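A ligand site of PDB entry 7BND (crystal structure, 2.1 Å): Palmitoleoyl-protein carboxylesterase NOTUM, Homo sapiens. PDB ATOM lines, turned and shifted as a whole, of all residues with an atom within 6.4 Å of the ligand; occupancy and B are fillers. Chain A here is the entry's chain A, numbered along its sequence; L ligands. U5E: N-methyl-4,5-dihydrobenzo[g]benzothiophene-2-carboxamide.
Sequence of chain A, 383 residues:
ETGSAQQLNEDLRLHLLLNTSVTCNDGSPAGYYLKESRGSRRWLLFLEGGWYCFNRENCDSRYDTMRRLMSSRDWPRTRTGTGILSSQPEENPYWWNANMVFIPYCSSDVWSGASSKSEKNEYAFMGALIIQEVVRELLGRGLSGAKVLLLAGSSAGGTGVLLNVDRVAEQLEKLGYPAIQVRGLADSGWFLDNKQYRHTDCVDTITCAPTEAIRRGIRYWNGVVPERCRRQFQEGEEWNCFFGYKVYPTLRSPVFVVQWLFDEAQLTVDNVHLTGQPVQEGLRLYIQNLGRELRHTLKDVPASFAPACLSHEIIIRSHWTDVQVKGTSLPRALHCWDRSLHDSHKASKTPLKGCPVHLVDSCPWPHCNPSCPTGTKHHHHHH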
ATOM      1  N   GLY A  49      24.038 -13.644 -10.835  1.00  0.00           N
ATOM      2  CA  GLY A  49      24.196 -12.812 -12.001  1.00  0.00           C
ATOM      3  C   GLY A  49      22.895 -12.595 -12.755  1.00  0.00           C
ATOM      4  O   GLY A  49      21.803 -12.928 -12.280  1.00  0.00           O
ATOM      5  N   GLY A  50      23.023 -12.043 -13.956  1.00  0.00           N
ATOM      6  CA  GLY A  50      21.864 -11.804 -14.803  1.00  0.00           C
ATOM      7  C   GLY A  50      21.853 -10.455 -15.499  1.00  0.00           C
ATOM      8  O   GLY A  50      20.836  -9.750 -15.469  1.00  0.00           O
ATOM      9  N   TRP A  51      22.964 -10.092 -16.127  1.00  0.00           N
ATOM     10  CA  TRP A  51      23.088  -8.884 -16.972  1.00  0.00           C
ATOM     11  C   TRP A  51      22.862  -7.651 -16.102  1.00  0.00           C
ATOM     12  O   TRP A  51      23.317  -7.605 -14.944  1.00  0.00           O
ATOM     13  CB  TRP A  51      22.159  -9.013 -18.172  1.00  0.00           C
ATOM     14  CG  TRP A  51      22.633 -10.011 -19.190  1.00  0.00           C
ATOM     15  CD1 TRP A  51      22.156 -11.280 -19.378  1.00  0.00           C
ATOM     16  CD2 TRP A  51      23.678  -9.838 -20.148  1.00  0.00           C
ATOM     17  NE1 TRP A  51      22.834 -11.896 -20.401  1.00  0.00           N
ATOM     18  CE2 TRP A  51      23.780 -11.038 -20.891  1.00  0.00           C
ATOM     19  CE3 TRP A  51      24.549  -8.783 -20.461  1.00  0.00           C
ATOM     20  CZ2 TRP A  51      24.703 -11.204 -21.911  1.00  0.00           C
ATOM     21  CZ3 TRP A  51      25.466  -8.958 -21.482  1.00  0.00           C
ATOM     22  CH2 TRP A  51      25.535 -10.165 -22.196  1.00  0.00           C
ATOM     23  N   TYR A  52      22.194  -6.618 -16.630  1.00  0.00           N
ATOM     24  CA  TYR A  52      22.035  -5.319 -15.966  1.00  0.00           C
ATOM     25  C   TYR A  52      21.121  -4.475 -16.847  1.00  0.00           C
ATOM     26  O   TYR A  52      20.673  -4.918 -17.907  1.00  0.00           O
ATOM     27  CB  TYR A  52      23.396  -4.641 -15.740  1.00  0.00           C
ATOM     28  CG  TYR A  52      24.306  -4.699 -16.938  1.00  0.00           C
ATOM     29  CD1 TYR A  52      24.293  -3.700 -17.900  1.00  0.00           C
ATOM     30  CD2 TYR A  52      25.194  -5.752 -17.125  1.00  0.00           C
ATOM     31  CE1 TYR A  52      25.127  -3.749 -19.003  1.00  0.00           C
ATOM     32  CE2 TYR A  52      26.030  -5.814 -18.222  1.00  0.00           C
ATOM     33  CZ  TYR A  52      25.993  -4.805 -19.154  1.00  0.00           C
ATOM     34  OH  TYR A  52      26.829  -4.867 -20.251  1.00  0.00           O
ATOM     35  N   TYR A 105      20.287 -11.442  -7.023  1.00  0.00           N
ATOM     36  CA  TYR A 105      20.687 -10.254  -7.763  1.00  0.00           C
ATOM     37  C   TYR A 105      19.431  -9.472  -8.117  1.00  0.00           C
ATOM     38  O   TYR A 105      18.687  -9.845  -9.025  1.00  0.00           O
ATOM     39  CB  TYR A 105      21.465 -10.683  -9.007  1.00  0.00           C
ATOM     40  CG  TYR A 105      21.981  -9.567  -9.895  1.00  0.00           C
ATOM     41  CD1 TYR A 105      22.622  -8.455  -9.367  1.00  0.00           C
ATOM     42  CD2 TYR A 105      21.840  -9.640 -11.270  1.00  0.00           C
ATOM     43  CE1 TYR A 105      23.096  -7.438 -10.189  1.00  0.00           C
ATOM     44  CE2 TYR A 105      22.310  -8.643 -12.101  1.00  0.00           C
ATOM     45  CZ  TYR A 105      22.930  -7.543 -11.561  1.00  0.00           C
ATOM     46  OH  TYR A 105      23.395  -6.556 -12.393  1.00  0.00           O
ATOM     47  N   VAL A 110      25.394  -4.727 -11.655  1.00  0.00           N
ATOM     48  CA  VAL A 110      26.618  -5.518 -11.573  1.00  0.00           C
ATOM     49  C   VAL A 110      27.186  -5.358 -10.153  1.00  0.00           C
ATOM     50  O   VAL A 110      28.407  -5.303  -9.962  1.00  0.00           O
ATOM     51  CB  VAL A 110      27.632  -5.103 -12.663  1.00  0.00           C
ATOM     52  CG1 VAL A 110      28.756  -6.126 -12.779  1.00  0.00           C
ATOM     53  CG2 VAL A 110      26.934  -4.943 -14.002  1.00  0.00           C
ATOM     54  N   SER A 154      28.715 -15.629 -10.177  1.00  0.00           N
ATOM     55  CA  SER A 154      28.737 -16.048 -11.573  1.00  0.00           C
ATOM     56  C   SER A 154      28.192 -14.949 -12.473  1.00  0.00           C
ATOM     57  O   SER A 154      27.232 -14.256 -12.118  1.00  0.00           O
ATOM     58  CB  SER A 154      27.920 -17.339 -11.784  1.00  0.00           C
ATOM     59  OG  SER A 154      28.430 -18.394 -10.991  1.00  0.00           O
ATOM     60  N   SER A 155      28.813 -14.787 -13.644  1.00  0.00           N
ATOM     61  CA  SER A 155      28.434 -13.794 -14.655  1.00  0.00           C
ATOM     62  C   SER A 155      28.515 -12.409 -14.014  1.00  0.00           C
ATOM     63  O   SER A 155      29.606 -12.018 -13.576  1.00  0.00           O
ATOM     64  CB  SER A 155      27.072 -14.162 -15.247  1.00  0.00           C
ATOM     65  OG  SER A 155      27.099 -15.455 -15.807  1.00  0.00           O
ATOM     66  N   ALA A 156      27.418 -11.651 -13.947  1.00  0.00           N
ATOM     67  CA  ALA A 156      27.466 -10.340 -13.308  1.00  0.00           C
ATOM     68  C   ALA A 156      27.852 -10.440 -11.839  1.00  0.00           C
ATOM     69  O   ALA A 156      28.508  -9.534 -11.310  1.00  0.00           O
ATOM     70  CB  ALA A 156      26.115  -9.631 -13.462  1.00  0.00           C
ATOM     71  N   GLY A 157      27.453 -11.528 -11.172  1.00  0.00           N
ATOM     72  CA  GLY A 157      27.946 -11.780  -9.832  1.00  0.00           C
ATOM     73  C   GLY A 157      29.431 -12.055  -9.782  1.00  0.00           C
ATOM     74  O   GLY A 157      30.086 -11.770  -8.784  1.00  0.00           O
ATOM     75  N   THR A 159      31.703 -10.590 -11.865  1.00  0.00           N
ATOM     76  CA  THR A 159      32.280  -9.251 -11.884  1.00  0.00           C
ATOM     77  C   THR A 159      32.068  -8.554 -10.548  1.00  0.00           C
ATOM     78  O   THR A 159      32.945  -7.825 -10.076  1.00  0.00           O
ATOM     79  CB  THR A 159      31.668  -8.432 -13.033  1.00  0.00           C
ATOM     80  OG1 THR A 159      31.725  -9.181 -14.251  1.00  0.00           O
ATOM     81  CG2 THR A 159      32.422  -7.129 -13.218  1.00  0.00           C
ATOM     82  N   SER A 188      32.928 -16.673 -14.671  1.00  0.00           N
ATOM     83  CA  SER A 188      32.332 -16.143 -15.908  1.00  0.00           C
ATOM     84  C   SER A 188      32.076 -14.641 -15.822  1.00  0.00           C
ATOM     85  O   SER A 188      31.125 -14.133 -16.411  1.00  0.00           O
ATOM     86  CB  SER A 188      31.052 -16.886 -16.273  1.00  0.00           C
ATOM     87  OG  SER A 188      31.286 -18.284 -16.345  1.00  0.00           O
ATOM     88  N   GLY A 189      32.934 -13.918 -15.100  1.00  0.00           N
ATOM     89  CA  GLY A 189      32.806 -12.478 -15.010  1.00  0.00           C
ATOM     90  C   GLY A 189      34.050 -11.748 -15.459  1.00  0.00           C
ATOM     91  O   GLY A 189      34.260 -10.576 -15.120  1.00  0.00           O
ATOM     92  N   PHE A 191      35.680 -10.406 -18.506  1.00  0.00           N
ATOM     93  CA  PHE A 191      35.346 -10.011 -19.873  1.00  0.00           C
ATOM     94  C   PHE A 191      36.441  -9.142 -20.486  1.00  0.00           C
ATOM     95  O   PHE A 191      37.245  -8.525 -19.783  1.00  0.00           O
ATOM     96  CB  PHE A 191      34.011  -9.265 -19.923  1.00  0.00           C
ATOM     97  CG  PHE A 191      32.851 -10.073 -19.407  1.00  0.00           C
ATOM     98  CD1 PHE A 191      32.228 -11.001 -20.219  1.00  0.00           C
ATOM     99  CD2 PHE A 191      32.401  -9.909 -18.106  1.00  0.00           C
ATOM    100  CE1 PHE A 191      31.159 -11.741 -19.747  1.00  0.00           C
ATOM    101  CE2 PHE A 191      31.333 -10.649 -17.634  1.00  0.00           C
ATOM    102  CZ  PHE A 191      30.714 -11.567 -18.458  1.00  0.00           C
ATOM    103  N   THR A 205      20.913  -4.524 -23.702  1.00  0.00           N
ATOM    104  CA  THR A 205      21.990  -4.986 -22.832  1.00  0.00           C
ATOM    105  C   THR A 205      22.722  -6.196 -23.392  1.00  0.00           C
ATOM    106  O   THR A 205      23.934  -6.336 -23.168  1.00  0.00           O
ATOM    107  CB  THR A 205      21.436  -5.328 -21.444  1.00  0.00           C
ATOM    108  OG1 THR A 205      20.696  -4.210 -20.939  1.00  0.00           O
ATOM    109  CG2 THR A 205      22.554  -5.661 -20.480  1.00  0.00           C
ATOM    110  N   PRO A 210      30.429  -3.901 -24.977  1.00  0.00           N
ATOM    111  CA  PRO A 210      30.606  -4.008 -23.526  1.00  0.00           C
ATOM    112  C   PRO A 210      31.123  -2.746 -22.883  1.00  0.00           C
ATOM    113  O   PRO A 210      30.839  -2.499 -21.703  1.00  0.00           O
ATOM    114  CB  PRO A 210      31.624  -5.163 -23.379  1.00  0.00           C
ATOM    115  CG  PRO A 210      32.246  -5.315 -24.733  1.00  0.00           C
ATOM    116  CD  PRO A 210      31.207  -4.908 -25.725  1.00  0.00           C
ATOM    117  N   THR A 211      31.879  -1.924 -23.615  1.00  0.00           N
ATOM    118  CA  THR A 211      32.362  -0.667 -23.051  1.00  0.00           C
ATOM    119  C   THR A 211      31.216   0.296 -22.813  1.00  0.00           C
ATOM    120  O   THR A 211      31.003   0.749 -21.672  1.00  0.00           O
ATOM    121  CB  THR A 211      33.389  -0.026 -23.969  1.00  0.00           C
ATOM    122  OG1 THR A 211      32.877   0.017 -25.307  1.00  0.00           O
ATOM    123  CG2 THR A 211      34.680  -0.791 -23.935  1.00  0.00           C
ATOM    124  N   ILE A 214      28.584  -0.230 -19.972  1.00  0.00           N
ATOM    125  CA  ILE A 214      29.048   0.031 -18.616  1.00  0.00           C
ATOM    126  C   ILE A 214      29.178   1.528 -18.383  1.00  0.00           C
ATOM    127  O   ILE A 214      28.848   2.030 -17.297  1.00  0.00           O
ATOM    128  CB  ILE A 214      30.378  -0.691 -18.342  1.00  0.00           C
ATOM    129  CG1 ILE A 214      30.227  -2.200 -18.562  1.00  0.00           C
ATOM    130  CG2 ILE A 214      30.870  -0.406 -16.933  1.00  0.00           C
ATOM    131  CD1 ILE A 214      29.193  -2.836 -17.664  1.00  0.00           C
ATOM    132  N   PHE A 242      35.451  -2.393 -14.390  1.00  0.00           N
ATOM    133  CA  PHE A 242      34.498  -3.483 -14.565  1.00  0.00           C
ATOM    134  C   PHE A 242      35.074  -4.618 -15.404  1.00  0.00           C
ATOM    135  O   PHE A 242      34.358  -5.592 -15.655  1.00  0.00           O
ATOM    136  CB  PHE A 242      33.215  -2.975 -15.218  1.00  0.00           C
ATOM    137  CG  PHE A 242      32.280  -2.295 -14.273  1.00  0.00           C
ATOM    138  CD1 PHE A 242      32.602  -1.061 -13.722  1.00  0.00           C
ATOM    139  CD2 PHE A 242      31.066  -2.878 -13.941  1.00  0.00           C
ATOM    140  CE1 PHE A 242      31.729  -0.432 -12.842  1.00  0.00           C
ATOM    141  CE2 PHE A 242      30.193  -2.249 -13.062  1.00  0.00           C
ATOM    142  CZ  PHE A 242      30.533  -1.025 -12.519  1.00  0.00           C
ATOM    143  N   PHE A 243      36.319  -4.517 -15.827  1.00  0.00           N
ATOM    144  CA  PHE A 243      36.935  -5.534 -16.686  1.00  0.00           C
ATOM    145  C   PHE A 243      38.067  -6.200 -15.915  1.00  0.00           C
ATOM    146  O   PHE A 243      39.044  -5.551 -15.548  1.00  0.00           O
ATOM    147  CB  PHE A 243      37.414  -4.904 -17.993  1.00  0.00           C
ATOM    148  CG  PHE A 243      36.288  -4.481 -18.888  1.00  0.00           C
ATOM    149  CD1 PHE A 243      35.715  -3.229 -18.770  1.00  0.00           C
ATOM    150  CD2 PHE A 243      35.769  -5.360 -19.831  1.00  0.00           C
ATOM    151  CE1 PHE A 243      34.663  -2.847 -19.579  1.00  0.00           C
ATOM    152  CE2 PHE A 243      34.723  -4.981 -20.648  1.00  0.00           C
ATOM    153  CZ  PHE A 243      34.162  -3.725 -20.522  1.00  0.00           C
ATOM    154  N   ALA A 265      28.408 -15.186 -23.114  1.00  0.00           N
ATOM    155  CA  ALA A 265      28.104 -13.771 -22.931  1.00  0.00           C
ATOM    156  C   ALA A 265      29.121 -12.892 -23.648  1.00  0.00           C
ATOM    157  O   ALA A 265      28.759 -11.846 -24.203  1.00  0.00           O
ATOM    158  CB  ALA A 265      28.045 -13.435 -21.446  1.00  0.00           C
ATOM    159  N   GLN A 266      30.387 -13.304 -23.646  1.00  0.00           N
ATOM    160  CA  GLN A 266      31.412 -12.554 -24.379  1.00  0.00           C
ATOM    161  C   GLN A 266      31.130 -12.568 -25.872  1.00  0.00           C
ATOM    162  O   GLN A 266      31.227 -11.538 -26.547  1.00  0.00           O
ATOM    163  CB  GLN A 266      32.797 -13.138 -24.082  1.00  0.00           C
ATOM    164  CG  GLN A 266      33.912 -12.481 -24.858  1.00  0.00           C
ATOM    165  CD  GLN A 266      34.360 -11.163 -24.249  1.00  0.00           C
ATOM    166  OE1 GLN A 266      34.686 -11.105 -23.065  1.00  0.00           O
ATOM    167  NE2 GLN A 266      34.354 -10.106 -25.054  1.00  0.00           N
ATOM    168  N   VAL A 269      27.970 -10.168 -26.698  1.00  0.00           N
ATOM    169  CA  VAL A 269      28.307  -8.751 -26.801  1.00  0.00           C
ATOM    170  C   VAL A 269      29.278  -8.492 -27.939  1.00  0.00           C
ATOM    171  O   VAL A 269      29.361  -7.361 -28.423  1.00  0.00           O
ATOM    172  CB  VAL A 269      28.871  -8.221 -25.470  1.00  0.00           C
ATOM    173  CG1 VAL A 269      27.888  -8.473 -24.331  1.00  0.00           C
ATOM    174  CG2 VAL A 269      30.219  -8.829 -25.167  1.00  0.00           C
ATOM    175  N   HIS A 312      28.608 -21.045 -20.382  1.00  0.00           N
ATOM    176  CA  HIS A 312      28.314 -19.884 -19.554  1.00  0.00           C
ATOM    177  C   HIS A 312      28.047 -20.359 -18.133  1.00  0.00           C
ATOM    178  O   HIS A 312      27.190 -21.212 -17.930  1.00  0.00           O
ATOM    179  CB  HIS A 312      27.105 -19.120 -20.090  1.00  0.00           C
ATOM    180  CG  HIS A 312      26.900 -17.779 -19.462  1.00  0.00           C
ATOM    181  ND1 HIS A 312      27.901 -16.830 -19.399  1.00  0.00           N
ATOM    182  CD2 HIS A 312      25.824 -17.235 -18.845  1.00  0.00           C
ATOM    183  CE1 HIS A 312      27.444 -15.748 -18.792  1.00  0.00           C
ATOM    184  NE2 HIS A 312      26.188 -15.973 -18.441  1.00  0.00           N
ATOM    185  N   GLU A 313      28.797 -19.810 -17.174  1.00  0.00           N
ATOM    186  CA  GLU A 313      28.689 -20.145 -15.753  1.00  0.00           C
ATOM    187  C   GLU A 313      29.077 -21.590 -15.478  1.00  0.00           C
ATOM    188  O   GLU A 313      29.127 -22.416 -16.399  1.00  0.00           O
ATOM    189  CB  GLU A 313      27.276 -19.885 -15.215  1.00  0.00           C
ATOM    190  CG  GLU A 313      26.777 -18.486 -15.443  1.00  0.00           C
ATOM    191  CD  GLU A 313      25.552 -18.160 -14.608  1.00  0.00           C
ATOM    192  OE1 GLU A 313      25.281 -16.955 -14.381  1.00  0.00           O
ATOM    193  OE2 GLU A 313      24.869 -19.105 -14.172  1.00  0.00           O
HETATM  194  C01 U5E L   1      24.152 -13.535 -17.450  1.00  0.00           C
HETATM  195  C03 U5E L   1      25.705 -11.587 -17.142  1.00  0.00           C
HETATM  196  C05 U5E L   1      26.756 -10.619 -17.691  1.00  0.00           C
HETATM  197  C06 U5E L   1      27.163 -10.481 -18.996  1.00  0.00           C
HETATM  198  C07 U5E L   1      28.157  -9.493 -19.241  1.00  0.00           C
HETATM  199  C08 U5E L   1      28.765  -9.170 -20.633  1.00  0.00           C
HETATM  200  C09 U5E L   1      29.331  -7.726 -20.710  1.00  0.00           C
HETATM  201  C10 U5E L   1      29.953  -7.253 -19.366  1.00  0.00           C
HETATM  202  C11 U5E L   1      30.959  -6.243 -19.359  1.00  0.00           C
HETATM  203  C12 U5E L   1      31.517  -5.833 -18.150  1.00  0.00           C
HETATM  204  C13 U5E L   1      31.101  -6.404 -16.958  1.00  0.00           C
HETATM  205  C14 U5E L   1      30.127  -7.387 -16.962  1.00  0.00           C
HETATM  206  C15 U5E L   1      29.547  -7.816 -18.195  1.00  0.00           C
HETATM  207  C16 U5E L   1      28.575  -8.806 -18.142  1.00  0.00           C
HETATM  208  N02 U5E L   1      25.144 -12.616 -17.989  1.00  0.00           N
HETATM  209  O04 U5E L   1      25.349 -11.502 -16.017  1.00  0.00           O
HETATM  210  S17 U5E L   1      27.674  -9.452 -16.807  1.00  0.00           S
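An oxygen (O04) of the ligand sits at hydrogen-bond distance from the backbone NH (N) of Trp 51.
O04 of the ligand sits at hydrogen-bond distance from N of Ala 156 (2.9 Å).
N of Gly 50 is in hydrogen-bond range of O04 of the ligand.
Tyr 52 touches the ligand.
Ser 155 touches the ligand (CB to O04, 3.3 Å).
Thr 159 touches the ligand.
Phe 191 touches the ligand (CE2 to C16, 3.4 Å).
Ile 214 touches the ligand (CD1 to C12, 3.8 Å).
O of Phe 242 touches C13 of the ligand, at 3.6 Å.
Ala 265 touches the ligand (CB to C06, 3.9 Å).
Val 269 touches the ligand (CG1 to C08, 3.9 Å).
His 312 touches the ligand (NE2 to C01, 3.3 Å).
Within 4 Å of the ligand: Gly 50, Trp 51, Tyr 52, Ser 155, Ala 156, Thr 159, Phe 191, Ile 214, Phe 242, Ala 265, Val 269 and His 312.
The side-chain hydroxyl (OH) of Tyr 105 sits at hydrogen-bond distance from the backbone carbonyl oxygen (O) of Trp 51, 2.8 Å away.
A ring nitrogen (NE2) of His 312 sits at hydrogen-bond distance from the side-chain hydroxyl (OG) of Ser 155, 2.8 Å away.
OG of Ser 155 sits at hydrogen-bond distance from OE1 of Glu 313, at 2.8 Å.
The side-chain hydroxyl of Thr 159 lies within hydrogen-bond range of the backbone carbonyl oxygen of Gly 189, 3.0 Å away.
OG1 of Thr 205 sits at hydrogen-bond distance from O of Tyr 52 (3.1 Å).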
